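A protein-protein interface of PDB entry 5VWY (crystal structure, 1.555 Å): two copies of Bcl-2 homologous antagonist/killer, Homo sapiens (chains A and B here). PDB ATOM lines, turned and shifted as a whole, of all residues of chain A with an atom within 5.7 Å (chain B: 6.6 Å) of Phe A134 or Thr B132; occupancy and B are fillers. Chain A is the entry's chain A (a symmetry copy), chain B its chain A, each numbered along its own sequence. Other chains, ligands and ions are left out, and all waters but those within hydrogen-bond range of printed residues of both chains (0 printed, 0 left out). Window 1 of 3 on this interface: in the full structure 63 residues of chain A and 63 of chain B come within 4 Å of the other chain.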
ATOM      1  N   GLU A  43      -0.024 -11.792 -37.517  1.00  0.00           N
ATOM      2  CA  GLU A  43       0.004 -10.414 -37.996  1.00  0.00           C
ATOM      3  C   GLU A  43       0.687 -10.317 -39.350  1.00  0.00           C
ATOM      4  O   GLU A  43       0.427  -9.378 -40.112  1.00  0.00           O
ATOM      5  CB  GLU A  43       0.735  -9.502 -37.011  1.00  0.00           C
ATOM      6  CG  GLU A  43       0.211  -9.533 -35.595  1.00  0.00           C
ATOM      7  CD  GLU A  43       0.773  -8.389 -34.770  1.00  0.00           C
ATOM      8  OE1 GLU A  43       1.889  -7.911 -35.089  1.00  0.00           O
ATOM      9  OE2 GLU A  43       0.093  -7.957 -33.817  1.00  0.00           O
ATOM     10  N   TYR A 127       5.842  -9.830 -30.998  1.00  0.00           N
ATOM     11  CA  TYR A 127       4.612 -10.618 -31.043  1.00  0.00           C
ATOM     12  C   TYR A 127       4.817 -12.010 -30.453  1.00  0.00           C
ATOM     13  O   TYR A 127       4.013 -12.473 -29.629  1.00  0.00           O
ATOM     14  CB  TYR A 127       4.063 -10.733 -32.468  1.00  0.00           C
ATOM     15  CG  TYR A 127       2.838 -11.630 -32.506  1.00  0.00           C
ATOM     16  CD1 TYR A 127       1.574 -11.126 -32.223  1.00  0.00           C
ATOM     17  CD2 TYR A 127       2.945 -12.992 -32.790  1.00  0.00           C
ATOM     18  CE1 TYR A 127       0.456 -11.938 -32.238  1.00  0.00           C
ATOM     19  CE2 TYR A 127       1.829 -13.822 -32.796  1.00  0.00           C
ATOM     20  CZ  TYR A 127       0.576 -13.292 -32.521  1.00  0.00           C
ATOM     21  OH  TYR A 127      -0.534 -14.113 -32.528  1.00  0.00           O
ATOM     22  N   THR A 132       3.513  -7.870 -26.841  1.00  0.00           N
ATOM     23  CA  THR A 132       2.679  -6.929 -27.580  1.00  0.00           C
ATOM     24  C   THR A 132       1.819  -6.064 -26.670  1.00  0.00           C
ATOM     25  O   THR A 132       1.271  -5.054 -27.126  1.00  0.00           O
ATOM     26  CB  THR A 132       1.811  -7.703 -28.576  1.00  0.00           C
ATOM     27  OG1 THR A 132       1.565  -9.025 -28.066  1.00  0.00           O
ATOM     28  CG2 THR A 132       2.523  -7.823 -29.909  1.00  0.00           C
ATOM     29  N   GLY A 133       1.707  -6.424 -25.401  1.00  0.00           N
ATOM     30  CA  GLY A 133       1.029  -5.588 -24.426  1.00  0.00           C
ATOM     31  C   GLY A 133      -0.483  -5.580 -24.493  1.00  0.00           C
ATOM     32  O   GLY A 133      -1.103  -4.721 -23.860  1.00  0.00           O
ATOM     33  N   PHE A 134      -1.112  -6.502 -25.222  1.00  0.00           N
ATOM     34  CA  PHE A 134      -2.554  -6.344 -25.366  1.00  0.00           C
ATOM     35  C   PHE A 134      -3.309  -6.769 -24.110  1.00  0.00           C
ATOM     36  O   PHE A 134      -4.284  -6.117 -23.721  1.00  0.00           O
ATOM     37  CB  PHE A 134      -3.090  -7.092 -26.580  1.00  0.00           C
ATOM     38  CG  PHE A 134      -4.524  -6.766 -26.853  1.00  0.00           C
ATOM     39  CD1 PHE A 134      -4.889  -5.475 -27.213  1.00  0.00           C
ATOM     40  CD2 PHE A 134      -5.511  -7.716 -26.683  1.00  0.00           C
ATOM     41  CE1 PHE A 134      -6.216  -5.148 -27.434  1.00  0.00           C
ATOM     42  CE2 PHE A 134      -6.843  -7.393 -26.889  1.00  0.00           C
ATOM     43  CZ  PHE A 134      -7.195  -6.112 -27.275  1.00  0.00           C
ATOM     44  N   LEU A 135      -2.888  -7.853 -23.465  1.00  0.00           N
ATOM     45  CA  LEU A 135      -3.505  -8.237 -22.199  1.00  0.00           C
ATOM     46  C   LEU A 135      -3.379  -7.118 -21.171  1.00  0.00           C
ATOM     47  O   LEU A 135      -4.329  -6.830 -20.426  1.00  0.00           O
ATOM     48  CB  LEU A 135      -2.850  -9.513 -21.685  1.00  0.00           C
ATOM     49  CG  LEU A 135      -3.250 -10.020 -20.307  1.00  0.00           C
ATOM     50  CD1 LEU A 135      -4.757 -10.296 -20.274  1.00  0.00           C
ATOM     51  CD2 LEU A 135      -2.470 -11.282 -20.009  1.00  0.00           C
ATOM     52  N   GLY A 136      -2.213  -6.480 -21.113  1.00  0.00           N
ATOM     53  CA  GLY A 136      -2.058  -5.328 -20.242  1.00  0.00           C
ATOM     54  C   GLY A 136      -3.004  -4.201 -20.605  1.00  0.00           C
ATOM     55  O   GLY A 136      -3.545  -3.524 -19.727  1.00  0.00           O
ATOM     56  N   GLN A 137      -3.235  -3.999 -21.906  1.00  0.00           N
ATOM     57  CA  GLN A 137      -4.218  -3.013 -22.337  1.00  0.00           C
ATOM     58  C   GLN A 137      -5.624  -3.400 -21.883  1.00  0.00           C
ATOM     59  O   GLN A 137      -6.373  -2.560 -21.371  1.00  0.00           O
ATOM     60  CB  GLN A 137      -4.161  -2.850 -23.856  1.00  0.00           C
ATOM     61  CG  GLN A 137      -4.901  -1.629 -24.366  1.00  0.00           C
ATOM     62  CD  GLN A 137      -4.323  -0.328 -23.833  1.00  0.00           C
ATOM     63  OE1 GLN A 137      -3.145  -0.034 -24.027  1.00  0.00           O
ATOM     64  NE2 GLN A 137      -5.150   0.450 -23.142  1.00  0.00           N
ATOM     65  N   VAL A 138      -6.007  -4.673 -22.064  1.00  0.00           N
ATOM     66  CA  VAL A 138      -7.321  -5.111 -21.601  1.00  0.00           C
ATOM     67  C   VAL A 138      -7.424  -4.971 -20.089  1.00  0.00           C
ATOM     68  O   VAL A 138      -8.482  -4.615 -19.562  1.00  0.00           O
ATOM     69  CB  VAL A 138      -7.617  -6.555 -22.060  1.00  0.00           C
ATOM     70  CG1 VAL A 138      -8.925  -7.061 -21.398  1.00  0.00           C
ATOM     71  CG2 VAL A 138      -7.740  -6.607 -23.564  1.00  0.00           C
ATOM     72  N   THR A 139      -6.332  -5.236 -19.366  1.00  0.00           N
ATOM     73  CA  THR A 139      -6.365  -5.062 -17.916  1.00  0.00           C
ATOM     74  C   THR A 139      -6.699  -3.623 -17.546  1.00  0.00           C
ATOM     75  O   THR A 139      -7.530  -3.378 -16.657  1.00  0.00           O
ATOM     76  CB  THR A 139      -5.035  -5.474 -17.299  1.00  0.00           C
ATOM     77  OG1 THR A 139      -4.761  -6.843 -17.605  1.00  0.00           O
ATOM     78  CG2 THR A 139      -5.063  -5.287 -15.792  1.00  0.00           C
ATOM     79  N   PHE A 141      -8.389  -1.566 -19.459  1.00  0.00           N
ATOM     80  CA  PHE A 141      -9.813  -1.438 -19.784  1.00  0.00           C
ATOM     81  C   PHE A 141     -10.672  -1.866 -18.607  1.00  0.00           C
ATOM     82  O   PHE A 141     -11.651  -1.197 -18.252  1.00  0.00           O
ATOM     83  CB  PHE A 141     -10.199  -2.315 -20.979  1.00  0.00           C
ATOM     84  CG  PHE A 141      -9.543  -1.942 -22.279  1.00  0.00           C
ATOM     85  CD1 PHE A 141      -8.821  -0.774 -22.411  1.00  0.00           C
ATOM     86  CD2 PHE A 141      -9.681  -2.780 -23.378  1.00  0.00           C
ATOM     87  CE1 PHE A 141      -8.228  -0.432 -23.634  1.00  0.00           C
ATOM     88  CE2 PHE A 141      -9.101  -2.455 -24.591  1.00  0.00           C
ATOM     89  CZ  PHE A 141      -8.369  -1.283 -24.720  1.00  0.00           C
ATOM     90  N   GLU B  43       1.324 -13.951 -23.838  1.00  0.00           N
ATOM     91  CA  GLU B  43       0.986 -12.853 -22.938  1.00  0.00           C
ATOM     92  C   GLU B  43       0.355 -13.370 -21.655  1.00  0.00           C
ATOM     93  O   GLU B  43       0.414 -12.697 -20.619  1.00  0.00           O
ATOM     94  CB  GLU B  43       0.018 -11.874 -23.601  1.00  0.00           C
ATOM     95  CG  GLU B  43       0.476 -11.316 -24.927  1.00  0.00           C
ATOM     96  CD  GLU B  43      -0.377 -10.135 -25.356  1.00  0.00           C
ATOM     97  OE1 GLU B  43      -1.561 -10.070 -24.945  1.00  0.00           O
ATOM     98  OE2 GLU B  43       0.139  -9.266 -26.088  1.00  0.00           O
ATOM     99  N   PRO B  86     -12.879  -7.785 -33.368  1.00  0.00           N
ATOM    100  CA  PRO B  86     -12.188  -6.799 -32.539  1.00  0.00           C
ATOM    101  C   PRO B  86     -10.723  -6.716 -32.921  1.00  0.00           C
ATOM    102  O   PRO B  86     -10.101  -7.700 -33.325  1.00  0.00           O
ATOM    103  CB  PRO B  86     -12.357  -7.348 -31.121  1.00  0.00           C
ATOM    104  CG  PRO B  86     -12.340  -8.837 -31.329  1.00  0.00           C
ATOM    105  CD  PRO B  86     -13.052  -9.069 -32.656  1.00  0.00           C
ATOM    106  N   THR B  87     -10.176  -5.516 -32.803  1.00  0.00           N
ATOM    107  CA  THR B  87      -8.765  -5.266 -33.032  1.00  0.00           C
ATOM    108  C   THR B  87      -8.242  -4.454 -31.859  1.00  0.00           C
ATOM    109  O   THR B  87      -9.012  -3.955 -31.037  1.00  0.00           O
ATOM    110  CB  THR B  87      -8.545  -4.492 -34.327  1.00  0.00           C
ATOM    111  OG1 THR B  87      -9.135  -3.197 -34.190  1.00  0.00           O
ATOM    112  CG2 THR B  87      -9.180  -5.216 -35.510  1.00  0.00           C
ATOM    113  N   ALA B  88      -6.924  -4.286 -31.791  1.00  0.00           N
ATOM    114  CA  ALA B  88      -6.375  -3.388 -30.782  1.00  0.00           C
ATOM    115  C   ALA B  88      -6.888  -1.967 -30.973  1.00  0.00           C
ATOM    116  O   ALA B  88      -7.013  -1.219 -29.997  1.00  0.00           O
ATOM    117  CB  ALA B  88      -4.843  -3.412 -30.825  1.00  0.00           C
ATOM    118  N   GLU B  89      -7.213  -1.590 -32.213  1.00  0.00           N
ATOM    119  CA  GLU B  89      -7.650  -0.228 -32.500  1.00  0.00           C
ATOM    120  C   GLU B  89      -9.061   0.037 -31.987  1.00  0.00           C
ATOM    121  O   GLU B  89      -9.345   1.125 -31.474  1.00  0.00           O
ATOM    122  CB  GLU B  89      -7.568   0.029 -34.008  1.00  0.00           C
ATOM    123  CG  GLU B  89      -7.994   1.420 -34.455  1.00  0.00           C
ATOM    124  CD  GLU B  89      -7.708   1.667 -35.933  1.00  0.00           C
ATOM    125  OE1 GLU B  89      -7.436   0.691 -36.664  1.00  0.00           O
ATOM    126  OE2 GLU B  89      -7.752   2.839 -36.366  1.00  0.00           O
ATOM    127  N   ALA B  91     -10.791  -2.088 -29.773  1.00  0.00           N
ATOM    128  CA  ALA B  91     -11.170  -2.916 -28.622  1.00  0.00           C
ATOM    129  C   ALA B  91     -11.740  -2.074 -27.490  1.00  0.00           C
ATOM    130  O   ALA B  91     -12.689  -2.496 -26.814  1.00  0.00           O
ATOM    131  CB  ALA B  91      -9.967  -3.721 -28.125  1.00  0.00           C
ATOM    132  N   TYR B  92     -11.167  -0.890 -27.250  1.00  0.00           N
ATOM    133  CA  TYR B  92     -11.651  -0.054 -26.151  1.00  0.00           C
ATOM    134  C   TYR B  92     -13.105   0.347 -26.367  1.00  0.00           C
ATOM    135  O   TYR B  92     -13.938   0.260 -25.450  1.00  0.00           O
ATOM    136  CB  TYR B  92     -10.770   1.190 -25.998  1.00  0.00           C
ATOM    137  CG  TYR B  92     -11.346   2.159 -25.002  1.00  0.00           C
ATOM    138  CD1 TYR B  92     -11.241   1.914 -23.640  1.00  0.00           C
ATOM    139  CD2 TYR B  92     -12.027   3.293 -25.417  1.00  0.00           C
ATOM    140  CE1 TYR B  92     -11.779   2.788 -22.715  1.00  0.00           C
ATOM    141  CE2 TYR B  92     -12.571   4.174 -24.497  1.00  0.00           C
ATOM    142  CZ  TYR B  92     -12.445   3.912 -23.148  1.00  0.00           C
ATOM    143  OH  TYR B  92     -12.983   4.779 -22.225  1.00  0.00           O
ATOM    144  N   GLY B 119     -12.942  -9.985 -20.602  1.00  0.00           N
ATOM    145  CA  GLY B 119     -11.579  -9.478 -20.794  1.00  0.00           C
ATOM    146  C   GLY B 119     -10.628 -10.578 -21.227  1.00  0.00           C
ATOM    147  O   GLY B 119      -9.786 -10.381 -22.119  1.00  0.00           O
ATOM    148  N   LEU B 122     -11.514 -11.573 -24.904  1.00  0.00           N
ATOM    149  CA  LEU B 122     -11.128 -10.512 -25.828  1.00  0.00           C
ATOM    150  C   LEU B 122      -9.619 -10.464 -26.007  1.00  0.00           C
ATOM    151  O   LEU B 122      -9.126 -10.393 -27.138  1.00  0.00           O
ATOM    152  CB  LEU B 122     -11.660  -9.175 -25.315  1.00  0.00           C
ATOM    153  CG  LEU B 122     -11.284  -7.926 -26.114  1.00  0.00           C
ATOM    154  CD1 LEU B 122     -11.928  -7.974 -27.494  1.00  0.00           C
ATOM    155  CD2 LEU B 122     -11.746  -6.672 -25.373  1.00  0.00           C
ATOM    156  N   ALA B 123      -8.865 -10.531 -24.903  1.00  0.00           N
ATOM    157  CA  ALA B 123      -7.401 -10.504 -25.010  1.00  0.00           C
ATOM    158  C   ALA B 123      -6.880 -11.696 -25.801  1.00  0.00           C
ATOM    159  O   ALA B 123      -5.968 -11.566 -26.629  1.00  0.00           O
ATOM    160  CB  ALA B 123      -6.776 -10.506 -23.615  1.00  0.00           C
ATOM    161  N   LEU B 124      -7.437 -12.871 -25.545  1.00  0.00           N
ATOM    162  CA  LEU B 124      -6.996 -14.075 -26.236  1.00  0.00           C
ATOM    163  C   LEU B 124      -7.312 -14.005 -27.725  1.00  0.00           C
ATOM    164  O   LEU B 124      -6.469 -14.347 -28.570  1.00  0.00           O
ATOM    165  CB  LEU B 124      -7.656 -15.298 -25.606  1.00  0.00           C
ATOM    166  CG  LEU B 124      -7.323 -16.608 -26.313  1.00  0.00           C
ATOM    167  CD1 LEU B 124      -5.823 -16.850 -26.271  1.00  0.00           C
ATOM    168  CD2 LEU B 124      -8.088 -17.774 -25.676  1.00  0.00           C
ATOM    169  N   HIS B 125      -8.531 -13.582 -28.064  1.00  0.00           N
ATOM    170  CA  HIS B 125      -8.949 -13.560 -29.458  1.00  0.00           C
ATOM    171  C   HIS B 125      -8.128 -12.564 -30.253  1.00  0.00           C
ATOM    172  O   HIS B 125      -7.702 -12.858 -31.373  1.00  0.00           O
ATOM    173  CB  HIS B 125     -10.438 -13.220 -29.555  1.00  0.00           C
ATOM    174  CG  HIS B 125     -10.957 -13.243 -30.956  1.00  0.00           C
ATOM    175  ND1 HIS B 125     -11.617 -14.330 -31.488  1.00  0.00           N
ATOM    176  CD2 HIS B 125     -10.866 -12.332 -31.951  1.00  0.00           C
ATOM    177  CE1 HIS B 125     -11.933 -14.074 -32.745  1.00  0.00           C
ATOM    178  NE2 HIS B 125     -11.478 -12.872 -33.055  1.00  0.00           N
ATOM    179  N   VAL B 126      -7.903 -11.378 -29.694  1.00  0.00           N
ATOM    180  CA  VAL B 126      -7.147 -10.370 -30.429  1.00  0.00           C
ATOM    181  C   VAL B 126      -5.703 -10.823 -30.618  1.00  0.00           C
ATOM    182  O   VAL B 126      -5.119 -10.640 -31.700  1.00  0.00           O
ATOM    183  CB  VAL B 126      -7.256  -9.013 -29.710  1.00  0.00           C
ATOM    184  CG1 VAL B 126      -6.269  -7.976 -30.273  1.00  0.00           C
ATOM    185  CG2 VAL B 126      -8.708  -8.496 -29.779  1.00  0.00           C
ATOM    186  N   TYR B 127      -5.102 -11.440 -29.596  1.00  0.00           N
ATOM    187  CA  TYR B 127      -3.718 -11.880 -29.760  1.00  0.00           C
ATOM    188  C   TYR B 127      -3.607 -13.010 -30.780  1.00  0.00           C
ATOM    189  O   TYR B 127      -2.750 -12.972 -31.676  1.00  0.00           O
ATOM    190  CB  TYR B 127      -3.100 -12.318 -28.429  1.00  0.00           C
ATOM    191  CG  TYR B 127      -1.695 -12.857 -28.636  1.00  0.00           C
ATOM    192  CD1 TYR B 127      -0.602 -12.001 -28.687  1.00  0.00           C
ATOM    193  CD2 TYR B 127      -1.460 -14.220 -28.816  1.00  0.00           C
ATOM    194  CE1 TYR B 127       0.678 -12.480 -28.892  1.00  0.00           C
ATOM    195  CE2 TYR B 127      -0.178 -14.713 -29.035  1.00  0.00           C
ATOM    196  CZ  TYR B 127       0.898 -13.839 -29.070  1.00  0.00           C
ATOM    197  OH  TYR B 127       2.172 -14.326 -29.286  1.00  0.00           O
ATOM    198  N   GLN B 128      -4.445 -14.036 -30.660  1.00  0.00           N
ATOM    199  CA  GLN B 128      -4.213 -15.232 -31.462  1.00  0.00           C
ATOM    200  C   GLN B 128      -4.609 -15.043 -32.923  1.00  0.00           C
ATOM    201  O   GLN B 128      -4.072 -15.742 -33.795  1.00  0.00           O
ATOM    202  CB  GLN B 128      -4.946 -16.424 -30.846  1.00  0.00           C
ATOM    203  CG  GLN B 128      -6.433 -16.383 -30.990  1.00  0.00           C
ATOM    204  CD  GLN B 128      -7.118 -17.403 -30.106  1.00  0.00           C
ATOM    205  OE1 GLN B 128      -6.466 -18.217 -29.444  1.00  0.00           O
ATOM    206  NE2 GLN B 128      -8.440 -17.366 -30.092  1.00  0.00           N
ATOM    207  N   HIS B 129      -5.500 -14.102 -33.218  1.00  0.00           N
ATOM    208  CA  HIS B 129      -5.838 -13.772 -34.595  1.00  0.00           C
ATOM    209  C   HIS B 129      -4.921 -12.709 -35.175  1.00  0.00           C
ATOM    210  O   HIS B 129      -5.182 -12.219 -36.279  1.00  0.00           O
ATOM    211  CB  HIS B 129      -7.300 -13.329 -34.697  1.00  0.00           C
ATOM    212  CG  HIS B 129      -8.271 -14.458 -34.576  1.00  0.00           C
ATOM    213  ND1 HIS B 129      -8.487 -15.127 -33.391  1.00  0.00           N
ATOM    214  CD2 HIS B 129      -9.065 -15.056 -35.496  1.00  0.00           C
ATOM    215  CE1 HIS B 129      -9.379 -16.083 -33.584  1.00  0.00           C
ATOM    216  NE2 HIS B 129      -9.744 -16.061 -34.852  1.00  0.00           N
ATOM    217  N   GLY B 130      -3.851 -12.355 -34.468  1.00  0.00           N
ATOM    218  CA  GLY B 130      -2.912 -11.387 -34.991  1.00  0.00           C
ATOM    219  C   GLY B 130      -3.517 -10.020 -35.187  1.00  0.00           C
ATOM    220  O   GLY B 130      -3.098  -9.280 -36.085  1.00  0.00           O
ATOM    221  N   LEU B 131      -4.509  -9.670 -34.373  1.00  0.00           N
ATOM    222  CA  LEU B 131      -5.172  -8.378 -34.433  1.00  0.00           C
ATOM    223  C   LEU B 131      -4.608  -7.392 -33.423  1.00  0.00           C
ATOM    224  O   LEU B 131      -5.193  -6.323 -33.217  1.00  0.00           O
ATOM    225  CB  LEU B 131      -6.672  -8.564 -34.210  1.00  0.00           C
ATOM    226  CG  LEU B 131      -7.258  -9.620 -35.147  1.00  0.00           C
ATOM    227  CD1 LEU B 131      -8.654 -10.032 -34.713  1.00  0.00           C
ATOM    228  CD2 LEU B 131      -7.265  -9.098 -36.574  1.00  0.00           C
ATOM    229  N   THR B 132      -3.483  -7.735 -32.789  1.00  0.00           N
ATOM    230  CA  THR B 132      -2.870  -6.915 -31.750  1.00  0.00           C
ATOM    231  C   THR B 132      -2.281  -5.621 -32.293  1.00  0.00           C
ATOM    232  O   THR B 132      -1.972  -4.714 -31.510  1.00  0.00           O
ATOM    233  CB  THR B 132      -1.802  -7.739 -31.026  1.00  0.00           C
ATOM    234  OG1 THR B 132      -1.267  -8.723 -31.929  1.00  0.00           O
ATOM    235  CG2 THR B 132      -2.409  -8.453 -29.835  1.00  0.00           C
ATOM    236  N   GLY B 133      -2.137  -5.510 -33.604  1.00  0.00           N
ATOM    237  CA  GLY B 133      -1.720  -4.264 -34.225  1.00  0.00           C
ATOM    238  C   GLY B 133      -0.253  -3.917 -34.097  1.00  0.00           C
ATOM    239  O   GLY B 133       0.117  -2.776 -34.390  1.00  0.00           O
ATOM    240  N   PHE B 134       0.609  -4.846 -33.684  1.00  0.00           N
ATOM    241  CA  PHE B 134       1.975  -4.403 -33.437  1.00  0.00           C
ATOM    242  C   PHE B 134       2.758  -4.201 -34.731  1.00  0.00           C
ATOM    243  O   PHE B 134       3.532  -3.244 -34.846  1.00  0.00           O
ATOM    244  CB  PHE B 134       2.724  -5.354 -32.513  1.00  0.00           C
ATOM    245  CG  PHE B 134       4.048  -4.800 -32.090  1.00  0.00           C
ATOM    246  CD1 PHE B 134       4.107  -3.649 -31.314  1.00  0.00           C
ATOM    247  CD2 PHE B 134       5.226  -5.377 -32.519  1.00  0.00           C
ATOM    248  CE1 PHE B 134       5.325  -3.104 -30.945  1.00  0.00           C
ATOM    249  CE2 PHE B 134       6.449  -4.829 -32.165  1.00  0.00           C
ATOM    250  CZ  PHE B 134       6.499  -3.699 -31.368  1.00  0.00           C
ATOM    251  N   LEU B 135       2.583  -5.083 -35.710  1.00  0.00           N
ATOM    252  CA  LEU B 135       3.223  -4.873 -37.006  1.00  0.00           C
ATOM    253  C   LEU B 135       2.790  -3.546 -37.618  1.00  0.00           C
ATOM    254  O   LEU B 135       3.612  -2.812 -38.190  1.00  0.00           O
ATOM    255  CB  LEU B 135       2.872  -6.031 -37.934  1.00  0.00           C
ATOM    256  CG  LEU B 135       3.325  -5.949 -39.385  1.00  0.00           C
ATOM    257  CD1 LEU B 135       4.853  -5.829 -39.444  1.00  0.00           C
ATOM    258  CD2 LEU B 135       2.859  -7.193 -40.110  1.00  0.00           C
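Of the 11 printed residues of chain A, 8 touch a printed residue of chain B.
Printed residues of chain A that touch a printed residue of chain B: Glu A43, Tyr A127, Thr A132, Gly A133, Phe A134, Leu A135, Val A138 and Phe A141.
Hydrophobic or aromatic side chains of chain B within 4 Å of the printed part of chain A: Ala B91, Tyr B92, Ala B123, Val B126, Tyr B127, Phe B134 and Leu B135.
Among the printed residues, no Asp or Glu carboxylate lies within 4 Å of a Lys or Arg side-chain nitrogen of the other chain.
The side-chain hydroxyl of Thr A132 lies within hydrogen-bond range of the side-chain carboxylate of Glu B43.
The side-chain carboxylate of Glu B43 lies within hydrogen-bond range of the backbone NH of Gly A133 (3.3 Å).
The side-chain carboxylate (OE2) of Glu B43 lies within hydrogen-bond range of the backbone NH (N) of Phe A134.
The backbone NH of Leu A135 is in hydrogen-bond range of the side-chain carboxylate of Glu B43 (3.0 Å).
The side-chain hydroxyl (OH) of Tyr B127 lies within hydrogen-bond range of the backbone carbonyl oxygen (O) of Tyr A127.
The side-chain hydroxyl (OG1) of Thr B132 lies within hydrogen-bond range of the side-chain carboxylate (OE2) of Glu A43 (2.4 Å).
N of Gly B133 lies within hydrogen-bond range of OE2 of Glu A43, at 3.3 Å.
The backbone NH (N) of Phe B134 lies within hydrogen-bond range of the side-chain carboxylate (OE2) of Glu A43 (3.2 Å).
The side-chain carboxylate (OE1) of Glu A43 sits at hydrogen-bond distance from the backbone NH (N) of Leu B135 (3.0 Å).
N of Ala B88 sits at hydrogen-bond distance from O of Leu B131 (3.0 Å).
O of Val B126 is in hydrogen-bond range of N of Leu B131, at 2.9 Å.
The side-chain hydroxyl (OG1) of Thr A139 sits at hydrogen-bond distance from the backbone carbonyl oxygen (O) of Leu A135 (2.9 Å).
Among the printed residues, pairs that only touch across the chains: Glu A43 with Gly B130 (3.4 Å), Tyr A127 with Gln B128 (3.99 Å), Tyr A127 with Thr B132 (3.7 Å), Thr A132 with Tyr B127 (3.7 Å), Thr A132 with Phe B134 (3.6 Å), Phe A134 with Ala B88 (3.8 Å), Phe A134 with Ala B91 (3.8 Å), Phe A134 with Leu B122 (3.8 Å), Phe A134 with Ala B123 (3.7 Å), Phe A134 with Val B126 (3.3 Å), Phe A134 with Thr B132 (3.6 Å), Leu A135 with Ala B123 (3.9 Å), Val A138 with Gly B119 (3.5 Å), Phe A141 with Ala B91 (3.9 Å) and Phe A141 with Tyr B92 (3.7 Å).
Phe A134 touches just these residues of chain B: Glu B43 (3.2 Å), Ala B88 (3.8 Å), Ala B91 (3.8 Å), Leu B122 (3.8 Å), Ala B123 (3.7 Å), Val B126 (3.3 Å) and Thr B132 (3.6 Å).
Of the printed residues of chain B, Val A138 touches Gly B119.
Printed residues of chain A within 4 Å of Glu B43: Thr A132, Gly A133, Phe A134 and Leu A135.
Of the printed residues of chain A, Tyr B92 touches Phe A141.
Of the printed residues of chain A, Gly B119 touches Val A138 (3.5 Å).
His B125 touches none of the printed residues of chain A.
His B129 touches none of the printed residues of chain A.
Printed residues of chain A within 4 Å of Thr B132: Glu A43, Tyr A127 and Phe A134.
Of the printed residues of chain A, Leu B135 touches Glu A43 (3.0 Å).
The nearest residue of chain B that does not touch Phe A134 is Thr B87 (4.7 Å).
The nearest residue of chain A that does not touch Thr B132 is Thr A132 (4.4 Å).
The nearest printed residue of chain A that does not touch Val B126 is Tyr A127 (5.7 Å).
Glu A43 touches Thr B132, and with the chains exchanged Thr A132 touches Glu B43.
Glu A43 touches Phe B134, and with the chains exchanged Phe A134 touches Glu B43.
Glu A43 touches Leu B135, and with the chains exchanged Leu A135 touches Glu B43.
Tyr A127 touches Thr B132, and with the chains exchanged Thr A132 touches Tyr B127.
Of the 24 pairs that touch across the chains among the printed residues, 13 have their exchanged pair printed and touching as well.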
